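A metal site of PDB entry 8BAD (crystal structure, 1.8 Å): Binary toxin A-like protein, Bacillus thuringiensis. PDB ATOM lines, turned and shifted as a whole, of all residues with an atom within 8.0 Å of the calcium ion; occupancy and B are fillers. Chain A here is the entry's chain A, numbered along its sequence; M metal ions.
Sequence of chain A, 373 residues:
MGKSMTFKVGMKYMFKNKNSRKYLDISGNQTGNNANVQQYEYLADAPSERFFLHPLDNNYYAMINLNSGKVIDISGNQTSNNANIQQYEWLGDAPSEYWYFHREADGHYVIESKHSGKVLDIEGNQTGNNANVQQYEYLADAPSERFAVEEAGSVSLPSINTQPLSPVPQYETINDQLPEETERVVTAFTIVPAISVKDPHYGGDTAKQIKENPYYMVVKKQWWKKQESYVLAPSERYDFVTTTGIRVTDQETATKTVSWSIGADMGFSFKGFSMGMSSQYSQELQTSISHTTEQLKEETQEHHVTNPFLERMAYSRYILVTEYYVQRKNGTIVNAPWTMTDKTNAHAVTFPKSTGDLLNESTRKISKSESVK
The backbone NH (N) of Glu 123 sits at hydrogen-bond distance from the backbone carbonyl oxygen (O) of Asn 132 (3.0 Å). The backbone NH (N) of Ser 75 lies within hydrogen-bond range of the backbone carbonyl oxygen (O) of Asn 84 (3.0 Å). O of Asn 36 sits at hydrogen-bond distance from N of Ser 27.
Within 4 Å of the calcium ion: Asn 36, Val 37, Asn 84, Ile 85, Asn 132 and Val 133. Along chain A the residues within 4 Å of the calcium ion span positions 36 to 133. The nearest printed residue that does not touch the calcium ion is Gln 86 (4.7 Å).
The side-chain amide oxygen (OD1) of Asn 132 binds the calcium ion (2.3 Å). The side-chain amide oxygen (OD1) of Asn 36 is bound to the calcium ion (2.4 Å). The calcium ion is bound by O of Ile 85, 2.4 Å away. OD1 of Asn 84 binds the calcium ion (2.5 Å). The backbone carbonyl oxygen (O) of Val 37 binds the calcium ion (2.5 Å). The backbone carbonyl oxygen (O) of Val 133 binds the calcium ion.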
ATOM      1  N   ASP A  25       4.289  36.910  -2.845  1.00  0.00           N
ATOM      2  CA  ASP A  25       3.689  37.745  -1.782  1.00  0.00           C
ATOM      3  C   ASP A  25       3.967  37.099  -0.423  1.00  0.00           C
ATOM      4  O   ASP A  25       4.209  35.875  -0.353  1.00  0.00           O
ATOM      5  CB  ASP A  25       2.207  37.951  -2.082  1.00  0.00           C
ATOM      6  CG  ASP A  25       1.542  38.866  -1.116  1.00  0.00           C
ATOM      7  OD1 ASP A  25       2.122  39.940  -0.823  1.00  0.00           O
ATOM      8  OD2 ASP A  25       0.477  38.480  -0.604  1.00  0.00           O
ATOM      9  N   SER A  27       2.285  36.161   2.982  1.00  0.00           N
ATOM     10  CA  SER A  27       1.015  35.899   3.691  1.00  0.00           C
ATOM     11  C   SER A  27       0.779  36.983   4.747  1.00  0.00           C
ATOM     12  O   SER A  27       1.705  37.220   5.567  1.00  0.00           O
ATOM     13  CB  SER A  27       1.028  34.522   4.299  1.00  0.00           C
ATOM     14  OG  SER A  27       0.059  34.423   5.316  1.00  0.00           O
ATOM     15  N   ASN A  34       9.793  33.321   9.276  1.00  0.00           N
ATOM     16  CA  ASN A  34       9.051  32.071   8.988  1.00  0.00           C
ATOM     17  C   ASN A  34       7.663  32.394   8.418  1.00  0.00           C
ATOM     18  O   ASN A  34       6.931  31.443   8.173  1.00  0.00           O
ATOM     19  CB  ASN A  34       8.897  31.166  10.212  1.00  0.00           C
ATOM     20  CG  ASN A  34      10.222  30.820  10.861  1.00  0.00           C
ATOM     21  OD1 ASN A  34      10.489  31.238  11.976  1.00  0.00           O
ATOM     22  ND2 ASN A  34      11.033  30.040  10.169  1.00  0.00           N
ATOM     23  N   ALA A  35       7.332  33.665   8.139  1.00  0.00           N
ATOM     24  CA  ALA A  35       6.059  34.039   7.484  1.00  0.00           C
ATOM     25  C   ALA A  35       5.998  33.368   6.113  1.00  0.00           C
ATOM     26  O   ALA A  35       7.026  33.332   5.422  1.00  0.00           O
ATOM     27  CB  ALA A  35       5.889  35.535   7.391  1.00  0.00           C
ATOM     28  N   ASN A  36       4.851  32.847   5.727  1.00  0.00           N
ATOM     29  CA  ASN A  36       4.679  32.068   4.482  1.00  0.00           C
ATOM     30  C   ASN A  36       4.846  32.964   3.242  1.00  0.00           C
ATOM     31  O   ASN A  36       4.377  34.123   3.257  1.00  0.00           O
ATOM     32  CB  ASN A  36       3.338  31.363   4.417  1.00  0.00           C
ATOM     33  CG  ASN A  36       3.365  30.312   3.332  1.00  0.00           C
ATOM     34  OD1 ASN A  36       4.383  29.651   3.160  1.00  0.00           O
ATOM     35  ND2 ASN A  36       2.307  30.222   2.563  1.00  0.00           N
ATOM     36  N   VAL A  37       5.507  32.434   2.218  1.00  0.00           N
ATOM     37  CA  VAL A  37       5.506  33.011   0.850  1.00  0.00           C
ATOM     38  C   VAL A  37       4.408  32.317   0.050  1.00  0.00           C
ATOM     39  O   VAL A  37       4.400  31.087  -0.022  1.00  0.00           O
ATOM     40  CB  VAL A  37       6.885  32.917   0.180  1.00  0.00           C
ATOM     41  CG1 VAL A  37       6.872  33.458  -1.240  1.00  0.00           C
ATOM     42  CG2 VAL A  37       7.928  33.646   0.998  1.00  0.00           C
ATOM     43  N   GLN A  38       3.525  33.096  -0.539  1.00  0.00           N
ATOM     44  CA  GLN A  38       2.336  32.625  -1.286  1.00  0.00           C
ATOM     45  C   GLN A  38       2.294  33.385  -2.606  1.00  0.00           C
ATOM     46  O   GLN A  38       3.173  34.279  -2.817  1.00  0.00           O
ATOM     47  CB  GLN A  38       1.071  32.891  -0.457  1.00  0.00           C
ATOM     48  CG  GLN A  38       0.918  34.370  -0.108  1.00  0.00           C
ATOM     49  CD  GLN A  38      -0.416  34.711   0.524  1.00  0.00           C
ATOM     50  OE1 GLN A  38      -1.106  33.855   1.065  1.00  0.00           O
ATOM     51  NE2 GLN A  38      -0.790  35.995   0.446  1.00  0.00           N
ATOM     52  N   GLN A  39       1.302  33.095  -3.455  1.00  0.00           N
ATOM     53  CA  GLN A  39       0.957  33.987  -4.599  1.00  0.00           C
ATOM     54  C   GLN A  39      -0.302  34.758  -4.262  1.00  0.00           C
ATOM     55  O   GLN A  39      -1.150  34.253  -3.461  1.00  0.00           O
ATOM     56  CB  GLN A  39       0.858  33.221  -5.918  1.00  0.00           C
ATOM     57  CG  GLN A  39      -0.300  32.240  -5.971  1.00  0.00           C
ATOM     58  CD  GLN A  39      -0.365  31.560  -7.316  1.00  0.00           C
ATOM     59  OE1 GLN A  39       0.552  31.622  -8.143  1.00  0.00           O
ATOM     60  NE2 GLN A  39      -1.496  30.910  -7.554  1.00  0.00           N
ATOM     61  N   ASP A  73      13.469  32.417   1.520  1.00  0.00           N
ATOM     62  CA  ASP A  73      14.218  31.404   2.318  1.00  0.00           C
ATOM     63  C   ASP A  73      13.492  30.060   2.182  1.00  0.00           C
ATOM     64  O   ASP A  73      12.300  30.054   1.789  1.00  0.00           O
ATOM     65  CB  ASP A  73      14.338  31.874   3.767  1.00  0.00           C
ATOM     66  CG  ASP A  73      15.146  30.946   4.633  1.00  0.00           C
ATOM     67  OD1 ASP A  73      16.137  30.401   4.126  1.00  0.00           O
ATOM     68  OD2 ASP A  73      14.729  30.719   5.811  1.00  0.00           O
ATOM     69  N   SER A  75      12.124  26.912   4.366  1.00  0.00           N
ATOM     70  CA  SER A  75      11.766  26.389   5.701  1.00  0.00           C
ATOM     71  C   SER A  75      12.682  25.199   6.051  1.00  0.00           C
ATOM     72  O   SER A  75      12.785  24.252   5.232  1.00  0.00           O
ATOM     73  CB  SER A  75      10.302  26.036   5.744  1.00  0.00           C
ATOM     74  OG  SER A  75      10.060  25.054   6.708  1.00  0.00           O
ATOM     75  N   ASN A  82       8.892  19.917  -2.601  1.00  0.00           N
ATOM     76  CA  ASN A  82       7.680  20.317  -1.854  1.00  0.00           C
ATOM     77  C   ASN A  82       8.071  21.049  -0.582  1.00  0.00           C
ATOM     78  O   ASN A  82       7.168  21.434   0.135  1.00  0.00           O
ATOM     79  CB  ASN A  82       6.771  19.137  -1.504  1.00  0.00           C
ATOM     80  CG  ASN A  82       6.331  18.346  -2.720  1.00  0.00           C
ATOM     81  OD1 ASN A  82       6.593  17.145  -2.829  1.00  0.00           O
ATOM     82  ND2 ASN A  82       5.679  19.029  -3.652  1.00  0.00           N
ATOM     83  N   ALA A  83       9.363  21.275  -0.318  1.00  0.00           N
ATOM     84  CA  ALA A  83       9.811  22.053   0.850  1.00  0.00           C
ATOM     85  C   ALA A  83       9.218  23.452   0.745  1.00  0.00           C
ATOM     86  O   ALA A  83       9.205  24.042  -0.371  1.00  0.00           O
ATOM     87  CB  ALA A  83      11.312  22.102   0.968  1.00  0.00           C
ATOM     88  N   ASN A  84       8.753  23.984   1.870  1.00  0.00           N
ATOM     89  CA  ASN A  84       8.027  25.270   1.902  1.00  0.00           C
ATOM     90  C   ASN A  84       8.995  26.433   1.684  1.00  0.00           C
ATOM     91  O   ASN A  84      10.106  26.371   2.199  1.00  0.00           O
ATOM     92  CB  ASN A  84       7.309  25.482   3.225  1.00  0.00           C
ATOM     93  CG  ASN A  84       6.407  26.686   3.155  1.00  0.00           C
ATOM     94  OD1 ASN A  84       5.678  26.854   2.164  1.00  0.00           O
ATOM     95  ND2 ASN A  84       6.435  27.518   4.167  1.00  0.00           N
ATOM     96  N   ILE A  85       8.551  27.480   1.000  1.00  0.00           N
ATOM     97  CA  ILE A  85       9.272  28.779   0.863  1.00  0.00           C
ATOM     98  C   ILE A  85       8.619  29.806   1.809  1.00  0.00           C
ATOM     99  O   ILE A  85       7.385  29.884   1.854  1.00  0.00           O
ATOM    100  CB  ILE A  85       9.258  29.240  -0.607  1.00  0.00           C
ATOM    101  CG1 ILE A  85       9.913  28.181  -1.502  1.00  0.00           C
ATOM    102  CG2 ILE A  85       9.903  30.614  -0.783  1.00  0.00           C
ATOM    103  CD1 ILE A  85      11.352  27.890  -1.178  1.00  0.00           C
ATOM    104  N   GLN A  86       9.450  30.511   2.569  1.00  0.00           N
ATOM    105  CA  GLN A  86       9.052  31.446   3.638  1.00  0.00           C
ATOM    106  C   GLN A  86       9.914  32.693   3.506  1.00  0.00           C
ATOM    107  O   GLN A  86      10.758  32.727   2.567  1.00  0.00           O
ATOM    108  CB  GLN A  86       9.289  30.790   4.995  1.00  0.00           C
ATOM    109  CG  GLN A  86      10.760  30.473   5.247  1.00  0.00           C
ATOM    110  CD  GLN A  86      11.006  29.781   6.556  1.00  0.00           C
ATOM    111  OE1 GLN A  86      10.085  29.209   7.187  1.00  0.00           O
ATOM    112  NE2 GLN A  86      12.250  29.828   6.994  1.00  0.00           N
ATOM    113  N   GLN A  87       9.755  33.653   4.411  1.00  0.00           N
ATOM    114  CA  GLN A  87      10.760  34.717   4.588  1.00  0.00           C
ATOM    115  C   GLN A  87      11.531  34.460   5.881  1.00  0.00           C
ATOM    116  O   GLN A  87      10.999  33.771   6.807  1.00  0.00           O
ATOM    117  CB  GLN A  87      10.121  36.098   4.576  1.00  0.00           C
ATOM    118  CG  GLN A  87       9.249  36.398   5.783  1.00  0.00           C
ATOM    119  CD  GLN A  87       8.698  37.797   5.730  1.00  0.00           C
ATOM    120  OE1 GLN A  87       8.738  38.469   4.718  1.00  0.00           O
ATOM    121  NE2 GLN A  87       8.174  38.262   6.845  1.00  0.00           N
ATOM    122  N   ASP A 121       8.300  27.439  -7.079  1.00  0.00           N
ATOM    123  CA  ASP A 121       7.203  26.687  -7.702  1.00  0.00           C
ATOM    124  C   ASP A 121       5.904  27.028  -6.974  1.00  0.00           C
ATOM    125  O   ASP A 121       5.966  27.324  -5.775  1.00  0.00           O
ATOM    126  CB  ASP A 121       7.506  25.183  -7.672  1.00  0.00           C
ATOM    127  CG  ASP A 121       6.449  24.359  -8.343  1.00  0.00           C
ATOM    128  OD1 ASP A 121       6.017  24.772  -9.429  1.00  0.00           O
ATOM    129  OD2 ASP A 121       6.015  23.322  -7.746  1.00  0.00           O
ATOM    130  N   GLU A 123       2.750  25.300  -5.528  1.00  0.00           N
ATOM    131  CA  GLU A 123       2.268  23.963  -5.116  1.00  0.00           C
ATOM    132  C   GLU A 123       1.055  23.585  -5.970  1.00  0.00           C
ATOM    133  O   GLU A 123       0.132  24.418  -6.072  1.00  0.00           O
ATOM    134  CB  GLU A 123       1.919  23.986  -3.623  1.00  0.00           C
ATOM    135  CG  GLU A 123       1.557  22.627  -3.078  1.00  0.00           C
ATOM    136  CD  GLU A 123       0.868  22.679  -1.737  1.00  0.00           C
ATOM    137  OE1 GLU A 123       1.142  21.800  -0.895  1.00  0.00           O
ATOM    138  OE2 GLU A 123       0.036  23.597  -1.538  1.00  0.00           O
ATOM    139  N   ASN A 130      -3.447  32.994  -2.684  1.00  0.00           N
ATOM    140  CA  ASN A 130      -2.994  32.394  -1.408  1.00  0.00           C
ATOM    141  C   ASN A 130      -2.468  30.972  -1.632  1.00  0.00           C
ATOM    142  O   ASN A 130      -2.100  30.317  -0.638  1.00  0.00           O
ATOM    143  CB  ASN A 130      -4.102  32.446  -0.354  1.00  0.00           C
ATOM    144  CG  ASN A 130      -4.681  33.827  -0.176  1.00  0.00           C
ATOM    145  OD1 ASN A 130      -5.851  34.067  -0.473  1.00  0.00           O
ATOM    146  ND2 ASN A 130      -3.891  34.764   0.324  1.00  0.00           N
ATOM    147  N   ALA A 131      -2.387  30.503  -2.888  1.00  0.00           N
ATOM    148  CA  ALA A 131      -1.702  29.239  -3.221  1.00  0.00           C
ATOM    149  C   ALA A 131      -0.250  29.342  -2.754  1.00  0.00           C
ATOM    150  O   ALA A 131       0.381  30.434  -2.892  1.00  0.00           O
ATOM    151  CB  ALA A 131      -1.770  28.913  -4.688  1.00  0.00           C
ATOM    152  N   ASN A 132       0.241  28.264  -2.171  1.00  0.00           N
ATOM    153  CA  ASN A 132       1.547  28.204  -1.488  1.00  0.00           C
ATOM    154  C   ASN A 132       2.671  28.250  -2.521  1.00  0.00           C
ATOM    155  O   ASN A 132       2.568  27.583  -3.573  1.00  0.00           O
ATOM    156  CB  ASN A 132       1.637  26.952  -0.614  1.00  0.00           C
ATOM    157  CG  ASN A 132       2.887  26.972   0.223  1.00  0.00           C
ATOM    158  OD1 ASN A 132       3.203  27.995   0.826  1.00  0.00           O
ATOM    159  ND2 ASN A 132       3.626  25.870   0.226  1.00  0.00           N
ATOM    160  N   VAL A 133       3.768  28.931  -2.202  1.00  0.00           N
ATOM    161  CA  VAL A 133       5.032  28.826  -2.976  1.00  0.00           C
ATOM    162  C   VAL A 133       5.953  27.788  -2.295  1.00  0.00           C
ATOM    163  O   VAL A 133       6.157  27.897  -1.091  1.00  0.00           O
ATOM    164  CB  VAL A 133       5.688  30.205  -3.096  1.00  0.00           C
ATOM    165  CG1 VAL A 133       7.041  30.124  -3.788  1.00  0.00           C
ATOM    166  CG2 VAL A 133       4.742  31.167  -3.800  1.00  0.00           C
ATOM    167  N   GLN A 134       6.463  26.827  -3.060  1.00  0.00           N
ATOM    168  CA  GLN A 134       7.363  25.735  -2.559  1.00  0.00           C
ATOM    169  C   GLN A 134       8.597  25.706  -3.456  1.00  0.00           C
ATOM    170  O   GLN A 134       8.686  26.557  -4.347  1.00  0.00           O
ATOM    171  CB  GLN A 134       6.632  24.382  -2.601  1.00  0.00           C
ATOM    172  CG  GLN A 134       6.168  24.007  -3.998  1.00  0.00           C
ATOM    173  CD  GLN A 134       5.517  22.641  -4.099  1.00  0.00           C
ATOM    174  OE1 GLN A 134       5.034  22.091  -3.110  1.00  0.00           O
ATOM    175  NE2 GLN A 134       5.518  22.087  -5.292  1.00  0.00           N
ATOM    176  N   GLN A 135       9.491  24.743  -3.237  1.00  0.00           N
ATOM    177  CA  GLN A 135      10.558  24.409  -4.212  1.00  0.00           C
ATOM    178  C   GLN A 135      10.214  23.064  -4.816  1.00  0.00           C
ATOM    179  O   GLN A 135       9.537  22.222  -4.109  1.00  0.00           O
ATOM    180  CB  GLN A 135      11.954  24.439  -3.582  1.00  0.00           C
ATOM    181  CG  GLN A 135      12.230  23.297  -2.618  1.00  0.00           C
ATOM    182  CD  GLN A 135      13.607  23.389  -2.000  1.00  0.00           C
ATOM    183  OE1 GLN A 135      14.375  24.331  -2.220  1.00  0.00           O
ATOM    184  NE2 GLN A 135      13.966  22.377  -1.235  1.00  0.00           N
HETATM  185 CA    CA M   1       5.279  29.006   1.031  1.00  0.00          CA
